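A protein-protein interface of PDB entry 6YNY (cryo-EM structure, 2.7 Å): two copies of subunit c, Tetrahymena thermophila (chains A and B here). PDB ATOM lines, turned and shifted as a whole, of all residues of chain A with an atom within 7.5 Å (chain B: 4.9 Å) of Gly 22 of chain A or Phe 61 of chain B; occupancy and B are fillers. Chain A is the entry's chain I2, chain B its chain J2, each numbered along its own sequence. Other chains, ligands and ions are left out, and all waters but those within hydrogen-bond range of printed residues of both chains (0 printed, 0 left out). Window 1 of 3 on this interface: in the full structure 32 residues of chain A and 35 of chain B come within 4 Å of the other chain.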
ATOM      1  N   MET A  16       6.765  27.914  12.601  1.00  0.00           N
ATOM      2  CA  MET A  16       5.529  27.477  11.969  1.00  0.00           C
ATOM      3  C   MET A  16       4.801  28.608  11.255  1.00  0.00           C
ATOM      4  O   MET A  16       3.734  28.368  10.681  1.00  0.00           O
ATOM      5  CB  MET A  16       4.598  26.870  13.016  1.00  0.00           C
ATOM      6  CG  MET A  16       5.141  25.624  13.677  1.00  0.00           C
ATOM      7  SD  MET A  16       4.006  24.971  14.913  1.00  0.00           S
ATOM      8  CE  MET A  16       3.924  26.355  16.047  1.00  0.00           C
ATOM      9  N   LEU A  17       5.339  29.823  11.278  1.00  0.00           N
ATOM     10  CA  LEU A  17       4.728  30.932  10.563  1.00  0.00           C
ATOM     11  C   LEU A  17       4.993  30.830   9.063  1.00  0.00           C
ATOM     12  O   LEU A  17       4.042  30.881   8.273  1.00  0.00           O
ATOM     13  CB  LEU A  17       5.223  32.262  11.139  1.00  0.00           C
ATOM     14  CG  LEU A  17       4.849  33.538  10.390  1.00  0.00           C
ATOM     15  CD1 LEU A  17       3.347  33.730  10.407  1.00  0.00           C
ATOM     16  CD2 LEU A  17       5.552  34.731  11.009  1.00  0.00           C
ATOM     17  N   PRO A  18       6.247  30.689   8.617  1.00  0.00           N
ATOM     18  CA  PRO A  18       6.464  30.421   7.186  1.00  0.00           C
ATOM     19  C   PRO A  18       5.718  29.201   6.690  1.00  0.00           C
ATOM     20  O   PRO A  18       5.282  29.180   5.533  1.00  0.00           O
ATOM     21  CB  PRO A  18       7.982  30.232   7.086  1.00  0.00           C
ATOM     22  CG  PRO A  18       8.530  30.981   8.219  1.00  0.00           C
ATOM     23  CD  PRO A  18       7.522  30.891   9.328  1.00  0.00           C
ATOM     24  N   ILE A  19       5.562  28.178   7.531  1.00  0.00           N
ATOM     25  CA  ILE A  19       4.776  27.014   7.139  1.00  0.00           C
ATOM     26  C   ILE A  19       3.381  27.441   6.716  1.00  0.00           C
ATOM     27  O   ILE A  19       2.765  26.815   5.845  1.00  0.00           O
ATOM     28  CB  ILE A  19       4.739  25.987   8.286  1.00  0.00           C
ATOM     29  CG1 ILE A  19       6.162  25.527   8.621  1.00  0.00           C
ATOM     30  CG2 ILE A  19       3.870  24.799   7.909  1.00  0.00           C
ATOM     31  CD1 ILE A  19       6.247  24.529   9.755  1.00  0.00           C
ATOM     32  N   ALA A  20       2.862  28.509   7.317  1.00  0.00           N
ATOM     33  CA  ALA A  20       1.552  29.021   6.937  1.00  0.00           C
ATOM     34  C   ALA A  20       1.621  29.811   5.635  1.00  0.00           C
ATOM     35  O   ALA A  20       0.859  29.548   4.699  1.00  0.00           O
ATOM     36  CB  ALA A  20       0.987  29.885   8.063  1.00  0.00           C
ATOM     37  N   PHE A  21       2.531  30.785   5.563  1.00  0.00           N
ATOM     38  CA  PHE A  21       2.654  31.593   4.355  1.00  0.00           C
ATOM     39  C   PHE A  21       3.085  30.758   3.158  1.00  0.00           C
ATOM     40  O   PHE A  21       2.702  31.059   2.022  1.00  0.00           O
ATOM     41  CB  PHE A  21       3.640  32.732   4.596  1.00  0.00           C
ATOM     42  CG  PHE A  21       3.046  33.892   5.334  1.00  0.00           C
ATOM     43  CD1 PHE A  21       3.026  35.152   4.767  1.00  0.00           C
ATOM     44  CD2 PHE A  21       2.484  33.719   6.585  1.00  0.00           C
ATOM     45  CE1 PHE A  21       2.474  36.218   5.439  1.00  0.00           C
ATOM     46  CE2 PHE A  21       1.931  34.783   7.262  1.00  0.00           C
ATOM     47  CZ  PHE A  21       1.924  36.033   6.688  1.00  0.00           C
ATOM     48  N   GLY A  22       3.878  29.711   3.385  1.00  0.00           N
ATOM     49  CA  GLY A  22       4.248  28.838   2.286  1.00  0.00           C
ATOM     50  C   GLY A  22       3.056  28.112   1.701  1.00  0.00           C
ATOM     51  O   GLY A  22       3.002  27.872   0.493  1.00  0.00           O
ATOM     52  N   ALA A  23       2.087  27.754   2.544  1.00  0.00           N
ATOM     53  CA  ALA A  23       0.869  27.122   2.053  1.00  0.00           C
ATOM     54  C   ALA A  23       0.059  28.090   1.204  1.00  0.00           C
ATOM     55  O   ALA A  23      -0.423  27.734   0.123  1.00  0.00           O
ATOM     56  CB  ALA A  23       0.033  26.618   3.228  1.00  0.00           C
ATOM     57  N   LEU A  24      -0.100  29.325   1.681  1.00  0.00           N
ATOM     58  CA  LEU A  24      -0.850  30.316   0.920  1.00  0.00           C
ATOM     59  C   LEU A  24      -0.163  30.621  -0.403  1.00  0.00           C
ATOM     60  O   LEU A  24      -0.817  30.690  -1.449  1.00  0.00           O
ATOM     61  CB  LEU A  24      -1.013  31.587   1.748  1.00  0.00           C
ATOM     62  CG  LEU A  24      -1.932  32.658   1.171  1.00  0.00           C
ATOM     63  CD1 LEU A  24      -3.342  32.122   1.016  1.00  0.00           C
ATOM     64  CD2 LEU A  24      -1.919  33.884   2.057  1.00  0.00           C
ATOM     65  N   GLY A  25       1.157  30.806  -0.378  1.00  0.00           N
ATOM     66  CA  GLY A  25       1.884  31.013  -1.616  1.00  0.00           C
ATOM     67  C   GLY A  25       1.710  29.864  -2.587  1.00  0.00           C
ATOM     68  O   GLY A  25       1.724  30.063  -3.805  1.00  0.00           O
ATOM     69  N   THR A  26       1.548  28.647  -2.065  1.00  0.00           N
ATOM     70  CA  THR A  26       1.301  27.494  -2.922  1.00  0.00           C
ATOM     71  C   THR A  26      -0.090  27.560  -3.540  1.00  0.00           C
ATOM     72  O   THR A  26      -0.244  27.437  -4.761  1.00  0.00           O
ATOM     73  CB  THR A  26       1.478  26.205  -2.117  1.00  0.00           C
ATOM     74  OG1 THR A  26       2.873  25.903  -1.995  1.00  0.00           O
ATOM     75  CG2 THR A  26       0.751  25.038  -2.771  1.00  0.00           C
ATOM     76  N   GLY A  27      -1.116  27.751  -2.710  1.00  0.00           N
ATOM     77  CA  GLY A  27      -2.468  27.850  -3.235  1.00  0.00           C
ATOM     78  C   GLY A  27      -2.599  28.914  -4.304  1.00  0.00           C
ATOM     79  O   GLY A  27      -3.341  28.749  -5.275  1.00  0.00           O
ATOM     80  N   VAL A  28      -1.882  30.026  -4.138  1.00  0.00           N
ATOM     81  CA  VAL A  28      -1.936  31.102  -5.120  1.00  0.00           C
ATOM     82  C   VAL A  28      -1.181  30.714  -6.384  1.00  0.00           C
ATOM     83  O   VAL A  28      -1.623  31.004  -7.501  1.00  0.00           O
ATOM     84  CB  VAL A  28      -1.385  32.399  -4.505  1.00  0.00           C
ATOM     85  CG1 VAL A  28      -1.050  33.407  -5.587  1.00  0.00           C
ATOM     86  CG2 VAL A  28      -2.390  32.980  -3.528  1.00  0.00           C
ATOM     87  N   PHE A  55       7.438  26.152  -6.522  1.00  0.00           N
ATOM     88  CA  PHE A  55       7.176  25.535  -5.225  1.00  0.00           C
ATOM     89  C   PHE A  55       8.466  25.192  -4.493  1.00  0.00           C
ATOM     90  O   PHE A  55       8.556  25.353  -3.271  1.00  0.00           O
ATOM     91  CB  PHE A  55       6.319  24.284  -5.399  1.00  0.00           C
ATOM     92  CG  PHE A  55       6.123  23.510  -4.128  1.00  0.00           C
ATOM     93  CD1 PHE A  55       6.947  22.445  -3.809  1.00  0.00           C
ATOM     94  CD2 PHE A  55       5.120  23.862  -3.246  1.00  0.00           C
ATOM     95  CE1 PHE A  55       6.762  21.740  -2.638  1.00  0.00           C
ATOM     96  CE2 PHE A  55       4.932  23.162  -2.075  1.00  0.00           C
ATOM     97  CZ  PHE A  55       5.755  22.100  -1.769  1.00  0.00           C
ATOM     98  N   ILE A  58       9.523  27.732  -2.400  1.00  0.00           N
ATOM     99  CA  ILE A  58       8.707  27.916  -1.202  1.00  0.00           C
ATOM    100  C   ILE A  58       9.246  27.093  -0.039  1.00  0.00           C
ATOM    101  O   ILE A  58       9.504  27.627   1.047  1.00  0.00           O
ATOM    102  CB  ILE A  58       7.237  27.566  -1.497  1.00  0.00           C
ATOM    103  CG1 ILE A  58       6.619  28.611  -2.424  1.00  0.00           C
ATOM    104  CG2 ILE A  58       6.450  27.463  -0.192  1.00  0.00           C
ATOM    105  CD1 ILE A  58       5.222  28.271  -2.895  1.00  0.00           C
ATOM    106  N   GLU A  59       9.413  25.782  -0.232  1.00  0.00           N
ATOM    107  CA  GLU A  59       9.966  24.950   0.832  1.00  0.00           C
ATOM    108  C   GLU A  59      11.387  25.345   1.197  1.00  0.00           C
ATOM    109  O   GLU A  59      11.888  24.923   2.246  1.00  0.00           O
ATOM    110  CB  GLU A  59       9.938  23.476   0.433  1.00  0.00           C
ATOM    111  CG  GLU A  59       8.540  22.901   0.300  1.00  0.00           C
ATOM    112  CD  GLU A  59       8.461  21.430   0.671  1.00  0.00           C
ATOM    113  OE1 GLU A  59       9.438  20.897   1.237  1.00  0.00           O
ATOM    114  OE2 GLU A  59       7.413  20.805   0.394  1.00  0.00           O
ATOM    115  N   THR A  60      12.047  26.135   0.355  1.00  0.00           N
ATOM    116  CA  THR A  60      13.331  26.712   0.722  1.00  0.00           C
ATOM    117  C   THR A  60      13.260  27.456   2.044  1.00  0.00           C
ATOM    118  O   THR A  60      13.976  27.145   3.002  1.00  0.00           O
ATOM    119  CB  THR A  60      13.787  27.686  -0.359  1.00  0.00           C
ATOM    120  OG1 THR A  60      13.556  27.133  -1.660  1.00  0.00           O
ATOM    121  CG2 THR A  60      15.212  28.066  -0.162  1.00  0.00           C
ATOM    122  N   PHE A  61      12.375  28.443   2.106  1.00  0.00           N
ATOM    123  CA  PHE A  61      12.192  29.187   3.339  1.00  0.00           C
ATOM    124  C   PHE A  61      11.727  28.269   4.454  1.00  0.00           C
ATOM    125  O   PHE A  61      12.070  28.483   5.623  1.00  0.00           O
ATOM    126  CB  PHE A  61      11.200  30.316   3.088  1.00  0.00           C
ATOM    127  CG  PHE A  61      11.624  31.242   1.979  1.00  0.00           C
ATOM    128  CD1 PHE A  61      12.481  32.297   2.227  1.00  0.00           C
ATOM    129  CD2 PHE A  61      11.156  31.057   0.687  1.00  0.00           C
ATOM    130  CE1 PHE A  61      12.873  33.141   1.205  1.00  0.00           C
ATOM    131  CE2 PHE A  61      11.544  31.903  -0.336  1.00  0.00           C
ATOM    132  CZ  PHE A  61      12.401  32.947  -0.074  1.00  0.00           C
ATOM    133  N   ILE A  62      10.955  27.238   4.114  1.00  0.00           N
ATOM    134  CA  ILE A  62      10.453  26.332   5.138  1.00  0.00           C
ATOM    135  C   ILE A  62      11.621  25.654   5.842  1.00  0.00           C
ATOM    136  O   ILE A  62      11.809  25.795   7.056  1.00  0.00           O
ATOM    137  CB  ILE A  62       9.517  25.291   4.502  1.00  0.00           C
ATOM    138  CG1 ILE A  62       8.290  25.967   3.894  1.00  0.00           C
ATOM    139  CG2 ILE A  62       9.110  24.257   5.526  1.00  0.00           C
ATOM    140  CD1 ILE A  62       7.278  26.403   4.894  1.00  0.00           C
ATOM    141  N   LEU B  57       0.355  19.433  -1.952  1.00  0.00           N
ATOM    142  CA  LEU B  57       1.488  20.195  -1.441  1.00  0.00           C
ATOM    143  C   LEU B  57       1.095  21.028  -0.230  1.00  0.00           C
ATOM    144  O   LEU B  57       1.933  21.288   0.641  1.00  0.00           O
ATOM    145  CB  LEU B  57       2.052  21.090  -2.542  1.00  0.00           C
ATOM    146  CG  LEU B  57       3.112  20.443  -3.431  1.00  0.00           C
ATOM    147  CD1 LEU B  57       2.612  19.130  -4.006  1.00  0.00           C
ATOM    148  CD2 LEU B  57       3.493  21.393  -4.541  1.00  0.00           C
ATOM    149  N   ILE B  58      -0.164  21.461  -0.156  1.00  0.00           N
ATOM    150  CA  ILE B  58      -0.613  22.233   0.999  1.00  0.00           C
ATOM    151  C   ILE B  58      -0.632  21.356   2.244  1.00  0.00           C
ATOM    152  O   ILE B  58      -0.121  21.742   3.301  1.00  0.00           O
ATOM    153  CB  ILE B  58      -1.993  22.859   0.724  1.00  0.00           C
ATOM    154  CG1 ILE B  58      -1.870  23.962  -0.331  1.00  0.00           C
ATOM    155  CG2 ILE B  58      -2.595  23.398   2.016  1.00  0.00           C
ATOM    156  CD1 ILE B  58      -3.189  24.566  -0.750  1.00  0.00           C
ATOM    157  N   GLU B  59      -1.225  20.164   2.140  1.00  0.00           N
ATOM    158  CA  GLU B  59      -1.261  19.255   3.278  1.00  0.00           C
ATOM    159  C   GLU B  59       0.133  18.846   3.724  1.00  0.00           C
ATOM    160  O   GLU B  59       0.306  18.429   4.875  1.00  0.00           O
ATOM    161  CB  GLU B  59      -2.086  18.014   2.939  1.00  0.00           C
ATOM    162  CG  GLU B  59      -3.556  18.298   2.679  1.00  0.00           C
ATOM    163  CD  GLU B  59      -4.314  18.663   3.940  1.00  0.00           C
ATOM    164  OE1 GLU B  59      -3.760  18.477   5.044  1.00  0.00           O
ATOM    165  OE2 GLU B  59      -5.465  19.135   3.828  1.00  0.00           O
ATOM    166  N   THR B  60       1.130  18.951   2.844  1.00  0.00           N
ATOM    167  CA  THR B  60       2.505  18.685   3.251  1.00  0.00           C
ATOM    168  C   THR B  60       2.917  19.622   4.378  1.00  0.00           C
ATOM    169  O   THR B  60       3.415  19.182   5.421  1.00  0.00           O
ATOM    170  CB  THR B  60       3.446  18.838   2.056  1.00  0.00           C
ATOM    171  OG1 THR B  60       3.106  17.874   1.050  1.00  0.00           O
ATOM    172  CG2 THR B  60       4.892  18.647   2.480  1.00  0.00           C
ATOM    173  N   PHE B  61       2.715  20.924   4.179  1.00  0.00           N
ATOM    174  CA  PHE B  61       2.961  21.887   5.244  1.00  0.00           C
ATOM    175  C   PHE B  61       2.175  21.520   6.496  1.00  0.00           C
ATOM    176  O   PHE B  61       2.679  21.646   7.618  1.00  0.00           O
ATOM    177  CB  PHE B  61       2.581  23.289   4.772  1.00  0.00           C
ATOM    178  CG  PHE B  61       3.297  23.728   3.525  1.00  0.00           C
ATOM    179  CD1 PHE B  61       4.549  24.317   3.594  1.00  0.00           C
ATOM    180  CD2 PHE B  61       2.714  23.554   2.282  1.00  0.00           C
ATOM    181  CE1 PHE B  61       5.203  24.721   2.446  1.00  0.00           C
ATOM    182  CE2 PHE B  61       3.364  23.955   1.132  1.00  0.00           C
ATOM    183  CZ  PHE B  61       4.610  24.540   1.214  1.00  0.00           C
ATOM    184  N   ILE B  62       0.936  21.059   6.319  1.00  0.00           N
ATOM    185  CA  ILE B  62       0.099  20.692   7.460  1.00  0.00           C
ATOM    186  C   ILE B  62       0.748  19.564   8.251  1.00  0.00           C
ATOM    187  O   ILE B  62       1.054  19.707   9.441  1.00  0.00           O
ATOM    188  CB  ILE B  62      -1.309  20.298   6.985  1.00  0.00           C
ATOM    189  CG1 ILE B  62      -1.940  21.419   6.156  1.00  0.00           C
ATOM    190  CG2 ILE B  62      -2.194  19.959   8.170  1.00  0.00           C
ATOM    191  CD1 ILE B  62      -2.307  22.640   6.949  1.00  0.00           C
ATOM    192  N   PHE B  63       0.964  18.418   7.600  1.00  0.00           N
ATOM    193  CA  PHE B  63       1.626  17.308   8.275  1.00  0.00           C
ATOM    194  C   PHE B  63       2.991  17.723   8.801  1.00  0.00           C
ATOM    195  O   PHE B  63       3.413  17.282   9.876  1.00  0.00           O
ATOM    196  CB  PHE B  63       1.764  16.118   7.324  1.00  0.00           C
ATOM    197  CG  PHE B  63       0.455  15.594   6.797  1.00  0.00           C
ATOM    198  CD1 PHE B  63      -0.729  15.805   7.486  1.00  0.00           C
ATOM    199  CD2 PHE B  63       0.413  14.882   5.610  1.00  0.00           C
ATOM    200  CE1 PHE B  63      -1.927  15.318   6.998  1.00  0.00           C
ATOM    201  CE2 PHE B  63      -0.781  14.394   5.118  1.00  0.00           C
ATOM    202  CZ  PHE B  63      -1.954  14.612   5.814  1.00  0.00           C
ATOM    203  N   MET B  64       3.699  18.572   8.054  1.00  0.00           N
ATOM    204  CA  MET B  64       4.984  19.075   8.523  1.00  0.00           C
ATOM    205  C   MET B  64       4.819  19.879   9.807  1.00  0.00           C
ATOM    206  O   MET B  64       5.633  19.767  10.730  1.00  0.00           O
ATOM    207  CB  MET B  64       5.640  19.923   7.435  1.00  0.00           C
ATOM    208  CG  MET B  64       7.023  20.423   7.796  1.00  0.00           C
ATOM    209  SD  MET B  64       7.724  21.505   6.541  1.00  0.00           S
ATOM    210  CE  MET B  64       7.874  20.382   5.153  1.00  0.00           C
ATOM    211  N   SER B  65       3.766  20.695   9.881  1.00  0.00           N
ATOM    212  CA  SER B  65       3.551  21.534  11.055  1.00  0.00           C
ATOM    213  C   SER B  65       3.210  20.692  12.278  1.00  0.00           C
ATOM    214  O   SER B  65       3.912  20.739  13.294  1.00  0.00           O
ATOM    215  CB  SER B  65       2.444  22.550  10.772  1.00  0.00           C
ATOM    216  OG  SER B  65       2.306  23.466  11.844  1.00  0.00           O
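The backbone carbonyl oxygen (O) of Gly 22 of chain A sits at hydrogen-bond distance from the side-chain hydroxyl (OG1) of Thr 26 of chain A.
Among the printed residues, pairs that only touch across the chains: Met 16 of chain A with Ser 65 of chain B (3.8 Å), Ile 19 of chain A with Phe 61 of chain B (3.4 Å), Ile 19 of chain A with Ser 65 of chain B (3.9 Å), Gly 22 of chain A with Phe 61 of chain B (3.8 Å), Thr 26 of chain A with Ile 58 of chain B (3.7 Å), Thr 26 of chain A with Phe 61 of chain B (3.7 Å), Phe 55 of chain A with Leu 57 of chain B (3.2 Å), Phe 55 of chain A with Phe 61 of chain B (3.6 Å), Ile 58 of chain A with Phe 61 of chain B (3.7 Å), Glu 59 of chain A with Thr 60 of chain B (3.9 Å), Ile 62 of chain A with Phe 61 of chain B (3.6 Å) and Ile 62 of chain A with Met 64 of chain B (3.2 Å).
Of chain B, only Phe 61 (3.8 Å) comes within 4 Å of Gly 22 of chain A.
Of the printed residues of chain B, Thr 26 of chain A touches Ile 58 (3.7 Å) and Phe 61 (3.7 Å).
Printed residues of chain B within 4 Å of Phe 55 of chain A: Leu 57 and Phe 61.
Printed residues of chain B within 4 Å of Ile 58 of chain A: Phe 61.
Phe 61 of chain A touches none of the printed residues of chain B.
Phe 61 of chain B touches just these residues of chain A: Ile 19, Gly 22, Thr 26, Phe 55, Ile 58 and Ile 62.
Of the printed residues of chain A, Ser 65 of chain B touches Met 16 and Ile 19.
The nearest printed residue of chain B that does not touch Gly 22 of chain A is Ile 58 of chain B (6.3 Å).
The nearest printed residue of chain A that does not touch Ile 58 of chain B is Ala 23 of chain A (4.1 Å).
Hydrophobic or aromatic side chains of chain A that line the printed part of chain B: Met 16, Ile 19, Phe 55, Ile 58 and Ile 62.
Hydrophobic or aromatic side chains of chain B that line the printed part of chain A: Leu 57, Ile 58, Phe 61 and Met 64.
Among the printed residues, 12 pairs touch across the chains.
Among the printed residues, no Asp or Glu carboxylate lies within 4 Å of a Lys or Arg side-chain nitrogen of the other chain.
Ile 58 of chain A touches Phe 61 of chain B, but with the chains exchanged Phe 61 of chain A does not touch Ile 58 of chain B (13.6 Å).
Glu 59 of chain A touches Thr 60 of chain B, but with the chains exchanged Thr 60 of chain A does not touch Glu 59 of chain B (14.4 Å).
Ile 62 of chain A touches Phe 61 of chain B, but with the chains exchanged Phe 61 of chain A does not touch Ile 62 of chain B (13.1 Å).
Positions printed for both chains: 58, 59, 60, 61 and 62.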
